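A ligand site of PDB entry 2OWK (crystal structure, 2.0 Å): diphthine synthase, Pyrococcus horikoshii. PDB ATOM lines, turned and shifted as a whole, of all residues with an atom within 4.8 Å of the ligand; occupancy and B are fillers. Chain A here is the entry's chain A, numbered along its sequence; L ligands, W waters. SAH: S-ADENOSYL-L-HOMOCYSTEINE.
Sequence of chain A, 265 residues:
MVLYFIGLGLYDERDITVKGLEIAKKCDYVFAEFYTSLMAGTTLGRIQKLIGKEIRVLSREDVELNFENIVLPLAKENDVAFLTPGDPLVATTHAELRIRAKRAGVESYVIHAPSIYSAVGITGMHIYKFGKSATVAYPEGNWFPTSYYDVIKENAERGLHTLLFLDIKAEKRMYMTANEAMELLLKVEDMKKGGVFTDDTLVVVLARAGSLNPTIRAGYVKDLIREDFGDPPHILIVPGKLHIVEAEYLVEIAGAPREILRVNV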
ATOM      1  N   LEU A  10       1.960  16.317  18.306  1.00  0.00           N
ATOM      2  CA  LEU A  10       1.049  17.419  17.987  1.00  0.00           C
ATOM      3  C   LEU A  10       1.762  18.710  17.544  1.00  0.00           C
ATOM      4  O   LEU A  10       1.312  19.413  16.656  1.00  0.00           O
ATOM      5  CB  LEU A  10       0.220  17.715  19.231  1.00  0.00           C
ATOM      6  CG  LEU A  10      -0.785  16.604  19.553  1.00  0.00           C
ATOM      7  CD1 LEU A  10      -1.208  16.621  21.017  1.00  0.00           C
ATOM      8  CD2 LEU A  10      -2.068  16.709  18.727  1.00  0.00           C
ATOM      9  N   THR A  36       0.440  16.069   5.813  1.00  0.00           N
ATOM     10  CA  THR A  36      -0.838  15.683   6.420  1.00  0.00           C
ATOM     11  C   THR A  36      -1.233  16.595   7.576  1.00  0.00           C
ATOM     12  O   THR A  36      -2.408  16.700   7.911  1.00  0.00           O
ATOM     13  CB  THR A  36      -0.813  14.225   6.944  1.00  0.00           C
ATOM     14  OG1 THR A  36       0.344  14.029   7.760  1.00  0.00           O
ATOM     15  CG2 THR A  36      -0.800  13.249   5.777  1.00  0.00           C
ATOM     16  N   SER A  37      -0.255  17.245   8.197  1.00  0.00           N
ATOM     17  CA  SER A  37      -0.547  18.139   9.300  1.00  0.00           C
ATOM     18  C   SER A  37       0.590  19.135   9.467  1.00  0.00           C
ATOM     19  O   SER A  37       1.587  19.074   8.746  1.00  0.00           O
ATOM     20  CB  SER A  37      -0.738  17.349  10.599  1.00  0.00           C
ATOM     21  OG  SER A  37      -1.174  18.208  11.640  1.00  0.00           O
ATOM     22  N   LEU A  38       0.429  20.044  10.418  1.00  0.00           N
ATOM     23  CA  LEU A  38       1.438  21.056  10.697  1.00  0.00           C
ATOM     24  C   LEU A  38       1.938  21.004  12.138  1.00  0.00           C
ATOM     25  O   LEU A  38       1.152  21.082  13.077  1.00  0.00           O
ATOM     26  CB  LEU A  38       0.869  22.453  10.430  1.00  0.00           C
ATOM     27  CG  LEU A  38       1.742  23.640  10.837  1.00  0.00           C
ATOM     28  CD1 LEU A  38       3.031  23.631  10.033  1.00  0.00           C
ATOM     29  CD2 LEU A  38       0.986  24.947  10.625  1.00  0.00           C
ATOM     30  N   PRO A  85       3.429  13.692  11.287  1.00  0.00           N
ATOM     31  CA  PRO A  85       2.978  14.536  12.393  1.00  0.00           C
ATOM     32  C   PRO A  85       1.851  13.759  13.083  1.00  0.00           C
ATOM     33  O   PRO A  85       1.278  12.847  12.479  1.00  0.00           O
ATOM     34  CB  PRO A  85       2.446  15.783  11.688  1.00  0.00           C
ATOM     35  CG  PRO A  85       3.183  15.798  10.378  1.00  0.00           C
ATOM     36  CD  PRO A  85       3.198  14.351   9.988  1.00  0.00           C
ATOM     37  N   GLY A  86       1.531  14.123  14.325  1.00  0.00           N
ATOM     38  CA  GLY A  86       0.469  13.450  15.060  1.00  0.00           C
ATOM     39  C   GLY A  86       0.606  11.954  15.062  1.00  0.00           C
ATOM     40  O   GLY A  86       1.722  11.429  15.202  1.00  0.00           O
ATOM     41  N   ASP A  87      -0.519  11.244  14.948  1.00  0.00           N
ATOM     42  CA  ASP A  87      -0.514   9.786  14.888  1.00  0.00           C
ATOM     43  C   ASP A  87      -0.542   9.487  13.391  1.00  0.00           C
ATOM     44  O   ASP A  87      -1.353  10.032  12.649  1.00  0.00           O
ATOM     45  CB  ASP A  87      -1.746   9.213  15.577  1.00  0.00           C
ATOM     46  CG  ASP A  87      -1.784   7.696  15.534  1.00  0.00           C
ATOM     47  OD1 ASP A  87      -1.935   7.126  14.432  1.00  0.00           O
ATOM     48  OD2 ASP A  87      -1.668   7.071  16.608  1.00  0.00           O
ATOM     49  N   VAL A  90      -4.169   8.488  11.819  1.00  0.00           N
ATOM     50  CA  VAL A  90      -5.354   9.255  12.134  1.00  0.00           C
ATOM     51  C   VAL A  90      -5.599  10.375  11.118  1.00  0.00           C
ATOM     52  O   VAL A  90      -4.767  11.269  10.962  1.00  0.00           O
ATOM     53  CB  VAL A  90      -5.249   9.872  13.554  1.00  0.00           C
ATOM     54  CG1 VAL A  90      -6.457  10.748  13.835  1.00  0.00           C
ATOM     55  CG2 VAL A  90      -5.167   8.754  14.590  1.00  0.00           C
ATOM     56  N   ALA A  91      -6.720  10.305  10.434  1.00  0.00           N
ATOM     57  CA  ALA A  91      -7.074  11.326   9.447  1.00  0.00           C
ATOM     58  C   ALA A  91      -6.044  11.406   8.325  1.00  0.00           C
ATOM     59  O   ALA A  91      -5.716  12.487   7.850  1.00  0.00           O
ATOM     60  CB  ALA A  91      -7.247  12.687  10.123  1.00  0.00           C
ATOM     61  N   THR A  92      -5.511  10.249   7.942  1.00  0.00           N
ATOM     62  CA  THR A  92      -4.619  10.066   6.819  1.00  0.00           C
ATOM     63  C   THR A  92      -4.994   8.785   6.084  1.00  0.00           C
ATOM     64  O   THR A  92      -5.834   8.010   6.523  1.00  0.00           O
ATOM     65  CB  THR A  92      -3.178   9.959   7.335  1.00  0.00           C
ATOM     66  OG1 THR A  92      -2.981   8.660   7.916  1.00  0.00           O
ATOM     67  CG2 THR A  92      -2.896  11.030   8.402  1.00  0.00           C
ATOM     68  N   PRO A 114       0.695  11.391  20.277  1.00  0.00           N
ATOM     69  CA  PRO A 114      -0.539  12.150  20.556  1.00  0.00           C
ATOM     70  C   PRO A 114      -1.193  12.670  19.264  1.00  0.00           C
ATOM     71  O   PRO A 114      -0.516  13.152  18.364  1.00  0.00           O
ATOM     72  CB  PRO A 114      -0.062  13.264  21.490  1.00  0.00           C
ATOM     73  CG  PRO A 114       1.430  13.358  21.321  1.00  0.00           C
ATOM     74  CD  PRO A 114       1.847  11.949  21.007  1.00  0.00           C
ATOM     75  N   SER A 115      -2.520  12.520  19.201  1.00  0.00           N
ATOM     76  CA  SER A 115      -3.301  12.930  18.032  1.00  0.00           C
ATOM     77  C   SER A 115      -4.313  14.024  18.376  1.00  0.00           C
ATOM     78  O   SER A 115      -4.857  14.051  19.482  1.00  0.00           O
ATOM     79  CB  SER A 115      -4.064  11.714  17.484  1.00  0.00           C
ATOM     80  OG  SER A 115      -4.923  12.085  16.407  1.00  0.00           O
ATOM     81  N   ILE A 116      -4.567  14.916  17.429  1.00  0.00           N
ATOM     82  CA  ILE A 116      -5.538  15.979  17.662  1.00  0.00           C
ATOM     83  C   ILE A 116      -6.924  15.368  17.911  1.00  0.00           C
ATOM     84  O   ILE A 116      -7.755  15.949  18.611  1.00  0.00           O
ATOM     85  CB  ILE A 116      -5.609  16.955  16.447  1.00  0.00           C
ATOM     86  CG1 ILE A 116      -6.503  18.145  16.790  1.00  0.00           C
ATOM     87  CG2 ILE A 116      -6.143  16.221  15.217  1.00  0.00           C
ATOM     88  CD1 ILE A 116      -5.948  19.017  17.902  1.00  0.00           C
ATOM     89  N   TYR A 117      -7.161  14.192  17.355  1.00  0.00           N
ATOM     90  CA  TYR A 117      -8.431  13.502  17.516  1.00  0.00           C
ATOM     91  C   TYR A 117      -8.777  13.255  18.989  1.00  0.00           C
ATOM     92  O   TYR A 117      -9.939  13.340  19.377  1.00  0.00           O
ATOM     93  CB  TYR A 117      -8.413  12.178  16.728  1.00  0.00           C
ATOM     94  CG  TYR A 117      -9.698  11.389  16.727  1.00  0.00           C
ATOM     95  CD1 TYR A 117     -10.861  11.890  16.126  1.00  0.00           C
ATOM     96  CD2 TYR A 117      -9.740  10.123  17.291  1.00  0.00           C
ATOM     97  CE1 TYR A 117     -12.032  11.113  16.089  1.00  0.00           C
ATOM     98  CE2 TYR A 117     -10.897   9.357  17.268  1.00  0.00           C
ATOM     99  CZ  TYR A 117     -12.039   9.853  16.669  1.00  0.00           C
ATOM    100  OH  TYR A 117     -13.162   9.055  16.655  1.00  0.00           O
ATOM    101  N   PHE A 165     -11.738  18.823  11.197  1.00  0.00           N
ATOM    102  CA  PHE A 165     -10.339  18.941  10.829  1.00  0.00           C
ATOM    103  C   PHE A 165     -10.364  20.065   9.787  1.00  0.00           C
ATOM    104  O   PHE A 165     -11.307  20.171   9.013  1.00  0.00           O
ATOM    105  CB  PHE A 165      -9.852  17.654  10.164  1.00  0.00           C
ATOM    106  CG  PHE A 165      -9.776  16.480  11.107  1.00  0.00           C
ATOM    107  CD1 PHE A 165      -8.672  16.302  11.937  1.00  0.00           C
ATOM    108  CD2 PHE A 165     -10.801  15.533  11.143  1.00  0.00           C
ATOM    109  CE1 PHE A 165      -8.588  15.204  12.785  1.00  0.00           C
ATOM    110  CE2 PHE A 165     -10.728  14.427  11.995  1.00  0.00           C
ATOM    111  CZ  PHE A 165      -9.609  14.263  12.814  1.00  0.00           C
ATOM    112  N   LEU A 166      -9.339  20.908   9.784  1.00  0.00           N
ATOM    113  CA  LEU A 166      -9.296  22.005   8.821  1.00  0.00           C
ATOM    114  C   LEU A 166      -8.302  21.703   7.707  1.00  0.00           C
ATOM    115  O   LEU A 166      -7.294  21.019   7.919  1.00  0.00           O
ATOM    116  CB  LEU A 166      -8.963  23.316   9.542  1.00  0.00           C
ATOM    117  CG  LEU A 166      -9.954  23.655  10.663  1.00  0.00           C
ATOM    118  CD1 LEU A 166      -9.697  25.063  11.171  1.00  0.00           C
ATOM    119  CD2 LEU A 166     -11.400  23.541  10.155  1.00  0.00           C
ATOM    120  N   ASP A 167      -8.581  22.220   6.514  1.00  0.00           N
ATOM    121  CA  ASP A 167      -7.740  21.956   5.358  1.00  0.00           C
ATOM    122  C   ASP A 167      -6.301  22.466   5.474  1.00  0.00           C
ATOM    123  O   ASP A 167      -5.993  23.355   6.264  1.00  0.00           O
ATOM    124  CB  ASP A 167      -8.384  22.539   4.097  1.00  0.00           C
ATOM    125  CG  ASP A 167      -8.038  21.746   2.839  1.00  0.00           C
ATOM    126  OD1 ASP A 167      -7.223  20.800   2.924  1.00  0.00           O
ATOM    127  OD2 ASP A 167      -8.587  22.068   1.774  1.00  0.00           O
ATOM    128  N   ILE A 168      -5.423  21.863   4.674  1.00  0.00           N
ATOM    129  CA  ILE A 168      -4.021  22.237   4.644  1.00  0.00           C
ATOM    130  C   ILE A 168      -3.451  21.984   3.249  1.00  0.00           C
ATOM    131  O   ILE A 168      -3.722  20.968   2.618  1.00  0.00           O
ATOM    132  CB  ILE A 168      -3.188  21.422   5.674  1.00  0.00           C
ATOM    133  CG1 ILE A 168      -1.691  21.643   5.427  1.00  0.00           C
ATOM    134  CG2 ILE A 168      -3.542  19.949   5.586  1.00  0.00           C
ATOM    135  CD1 ILE A 168      -0.773  20.876   6.375  1.00  0.00           C
ATOM    136  N   LEU A 206      -9.613  25.251  18.990  1.00  0.00           N
ATOM    137  CA  LEU A 206      -8.411  24.748  19.656  1.00  0.00           C
ATOM    138  C   LEU A 206      -7.274  24.961  18.673  1.00  0.00           C
ATOM    139  O   LEU A 206      -7.275  24.406  17.574  1.00  0.00           O
ATOM    140  CB  LEU A 206      -8.547  23.258  19.978  1.00  0.00           C
ATOM    141  CG  LEU A 206      -7.308  22.586  20.589  1.00  0.00           C
ATOM    142  CD1 LEU A 206      -6.824  23.366  21.816  1.00  0.00           C
ATOM    143  CD2 LEU A 206      -7.635  21.149  20.953  1.00  0.00           C
ATOM    144  N   ALA A 207      -6.311  25.783  19.071  1.00  0.00           N
ATOM    145  CA  ALA A 207      -5.185  26.089  18.208  1.00  0.00           C
ATOM    146  C   ALA A 207      -3.861  25.709  18.856  1.00  0.00           C
ATOM    147  O   ALA A 207      -3.619  26.014  20.013  1.00  0.00           O
ATOM    148  CB  ALA A 207      -5.174  27.586  17.867  1.00  0.00           C
ATOM    149  N   ARG A 208      -3.025  25.032  18.073  1.00  0.00           N
ATOM    150  CA  ARG A 208      -1.705  24.599  18.522  1.00  0.00           C
ATOM    151  C   ARG A 208      -1.751  23.676  19.734  1.00  0.00           C
ATOM    152  O   ARG A 208      -1.011  23.846  20.705  1.00  0.00           O
ATOM    153  CB  ARG A 208      -0.839  25.830  18.829  1.00  0.00           C
ATOM    154  CG  ARG A 208      -0.714  26.793  17.649  1.00  0.00           C
ATOM    155  CD  ARG A 208       0.118  28.021  18.010  1.00  0.00           C
ATOM    156  NE  ARG A 208      -0.377  28.647  19.238  1.00  0.00           N
ATOM    157  CZ  ARG A 208      -1.501  29.336  19.339  1.00  0.00           C
ATOM    158  NH1 ARG A 208      -2.282  29.508  18.274  1.00  0.00           N
ATOM    159  NH2 ARG A 208      -1.877  29.830  20.514  1.00  0.00           N
ATOM    160  N   ALA A 209      -2.633  22.672  19.666  1.00  0.00           N
ATOM    161  CA  ALA A 209      -2.726  21.690  20.729  1.00  0.00           C
ATOM    162  C   ALA A 209      -1.340  21.069  20.811  1.00  0.00           C
ATOM    163  O   ALA A 209      -0.651  20.959  19.801  1.00  0.00           O
ATOM    164  CB  ALA A 209      -3.755  20.630  20.360  1.00  0.00           C
ATOM    165  N   PRO A 233      -1.541  25.202  13.573  1.00  0.00           N
ATOM    166  CA  PRO A 233      -2.825  24.689  13.076  1.00  0.00           C
ATOM    167  C   PRO A 233      -3.992  24.941  14.024  1.00  0.00           C
ATOM    168  O   PRO A 233      -3.799  25.133  15.230  1.00  0.00           O
ATOM    169  CB  PRO A 233      -2.545  23.206  12.901  1.00  0.00           C
ATOM    170  CG  PRO A 233      -1.677  22.906  14.085  1.00  0.00           C
ATOM    171  CD  PRO A 233      -0.721  24.099  14.123  1.00  0.00           C
ATOM    172  N   HIS A 234      -5.196  24.927  13.461  1.00  0.00           N
ATOM    173  CA  HIS A 234      -6.435  25.134  14.209  1.00  0.00           C
ATOM    174  C   HIS A 234      -7.396  24.006  13.883  1.00  0.00           C
ATOM    175  O   HIS A 234      -7.315  23.398  12.818  1.00  0.00           O
ATOM    176  CB  HIS A 234      -7.159  26.408  13.759  1.00  0.00           C
ATOM    177  CG  HIS A 234      -6.416  27.693  14.005  1.00  0.00           C
ATOM    178  ND1 HIS A 234      -6.940  28.917  13.640  1.00  0.00           N
ATOM    179  CD2 HIS A 234      -5.216  27.936  14.579  1.00  0.00           C
ATOM    180  CE1 HIS A 234      -6.090  29.865  13.978  1.00  0.00           C
ATOM    181  NE2 HIS A 234      -5.034  29.300  14.544  1.00  0.00           N
ATOM    182  N   ILE A 235      -8.319  23.746  14.795  1.00  0.00           N
ATOM    183  CA  ILE A 235      -9.397  22.775  14.559  1.00  0.00           C
ATOM    184  C   ILE A 235     -10.633  23.464  15.092  1.00  0.00           C
ATOM    185  O   ILE A 235     -10.554  24.250  16.036  1.00  0.00           O
ATOM    186  CB  ILE A 235      -9.247  21.435  15.309  1.00  0.00           C
ATOM    187  CG1 ILE A 235      -9.939  20.307  14.545  1.00  0.00           C
ATOM    188  CG2 ILE A 235      -9.746  21.573  16.706  1.00  0.00           C
ATOM    189  CD1 ILE A 235      -9.036  19.123  14.307  1.00  0.00           C
HETATM  190  N   SAH L   1      -2.677  12.334  11.924  1.00  0.00           N
HETATM  191  CA  SAH L   1      -2.858  13.743  12.477  1.00  0.00           C
HETATM  192  CB  SAH L   1      -3.914  14.610  11.863  1.00  0.00           C
HETATM  193  CG  SAH L   1      -3.868  14.883  10.361  1.00  0.00           C
HETATM  194  SD  SAH L   1      -5.263  16.018   9.978  1.00  0.00           S
HETATM  195  C   SAH L   1      -3.098  13.574  14.038  1.00  0.00           C
HETATM  196  O   SAH L   1      -3.111  12.422  14.521  1.00  0.00           O
HETATM  197  OXT SAH L   1      -3.251  14.671  14.705  1.00  0.00           O
HETATM  198  C5' SAH L   1      -4.434  17.550  10.072  1.00  0.00           C
HETATM  199  C4' SAH L   1      -5.429  18.642  10.626  1.00  0.00           C
HETATM  200  O4' SAH L   1      -5.737  18.286  12.001  1.00  0.00           O
HETATM  201  C3' SAH L   1      -4.893  20.031  10.655  1.00  0.00           C
HETATM  202  O3' SAH L   1      -5.114  20.676   9.415  1.00  0.00           O
HETATM  203  C2' SAH L   1      -5.677  20.626  11.848  1.00  0.00           C
HETATM  204  O2' SAH L   1      -6.983  21.069  11.467  1.00  0.00           O
HETATM  205  C1' SAH L   1      -5.672  19.494  12.889  1.00  0.00           C
HETATM  206  N9  SAH L   1      -4.589  19.454  13.698  1.00  0.00           N
HETATM  207  C8  SAH L   1      -3.460  18.651  13.772  1.00  0.00           C
HETATM  208  N7  SAH L   1      -2.635  18.949  14.733  1.00  0.00           N
HETATM  209  C5  SAH L   1      -3.239  20.048  15.399  1.00  0.00           C
HETATM  210  C6  SAH L   1      -2.830  20.825  16.547  1.00  0.00           C
HETATM  211  N6  SAH L   1      -1.687  20.617  17.225  1.00  0.00           N
HETATM  212  N1  SAH L   1      -3.692  21.833  16.903  1.00  0.00           N
HETATM  213  C2  SAH L   1      -4.863  22.091  16.247  1.00  0.00           C
HETATM  214  N3  SAH L   1      -5.291  21.375  15.148  1.00  0.00           N
HETATM  215  C4  SAH L   1      -4.436  20.372  14.781  1.00  0.00           C
HETATM  216  O   HOH W   1       0.533  18.048  13.702  1.00  0.00           O
HETATM  217  O   HOH W   2      -0.636  13.424  10.298  1.00  0.00           O
HETATM  218  O   HOH W   3      -0.946  16.501  15.151  1.00  0.00           O
HETATM  219  O   HOH W   4      -4.284  23.296   8.693  1.00  0.00           O
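The backbone carbonyl oxygen (O) of Thr 36 sits close to a sulfur (SD) of the ligand, at 3.6 Å. Merely in contact with the ligand: Ser 37, Gly 86, Ala 91, Thr 92, Phe 165, Leu 206, Pro 233 and Ile 235. Hydrophobic or aromatic side chains that line the ligand: Val 90, Ala 91, Ile 116, Phe 165, Leu 166, Ala 209, Pro 233 and Ile 235. Within 4 Å of the ligand: Leu 10, Thr 36, Ser 37, Gly 86, Asp 87, Val 90, Ala 91, Thr 92, Ser 115, Ile 116, Phe 165, Leu 166, Leu 206, Arg 208, Ala 209, Pro 233, His 234 and Ile 235. The nearest printed residue that does not touch the ligand is Pro 85 (4.03 Å).
Water W2 lies within hydrogen-bond range of OG1 of Thr 36 (2.8 Å), N of the ligand (2.8 Å) and O of Pro 85 (3.0 Å). Water W4 lies within hydrogen-bond range of O3' of the ligand (2.8 Å) and O of Asp 167 (3.0 Å).
The backbone carbonyl oxygen (O) of Leu 166 is in hydrogen-bond range of an oxygen (O3') of the ligand (2.7 Å). O2' of the ligand is in hydrogen-bond range of O of His 234 (2.7 Å). O of Asp 87 lies within hydrogen-bond range of N of the ligand, 2.8 Å away. The backbone carbonyl oxygen of Leu 10 lies within hydrogen-bond range of a nitrogen (N6) of the ligand, 3.3 Å away. The backbone NH (N) of Ala 209 is in hydrogen-bond range of a nitrogen (N1) of the ligand (3.1 Å). The backbone NH (N) of Arg 208 lies within hydrogen-bond range of a nitrogen (N1) of the ligand (3.5 Å). The backbone NH (N) of Asp 87 is in hydrogen-bond range of an oxygen (O) of the ligand, at 2.9 Å. N of Ile 116 sits at hydrogen-bond distance from OXT of the ligand (3.0 Å). A nitrogen (N) of the ligand sits at hydrogen-bond distance from the backbone carbonyl oxygen (O) of Val 90. N of Leu 166 is in hydrogen-bond range of O2' of the ligand (2.9 Å). The side-chain hydroxyl (OG) of Ser 115 is in hydrogen-bond range of an oxygen (O) of the ligand, 2.6 Å away. O of Ala 209 sits at hydrogen-bond distance from N6 of the ligand (2.8 Å).
The side-chain hydroxyl of Ser 115 lies close to the backbone NH of Tyr 117 (3.2 Å). O of Pro 233 lies within hydrogen-bond range of N of Arg 208 (2.9 Å). O of Leu 206 sits at hydrogen-bond distance from N of Ile 235, at 3.0 Å.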
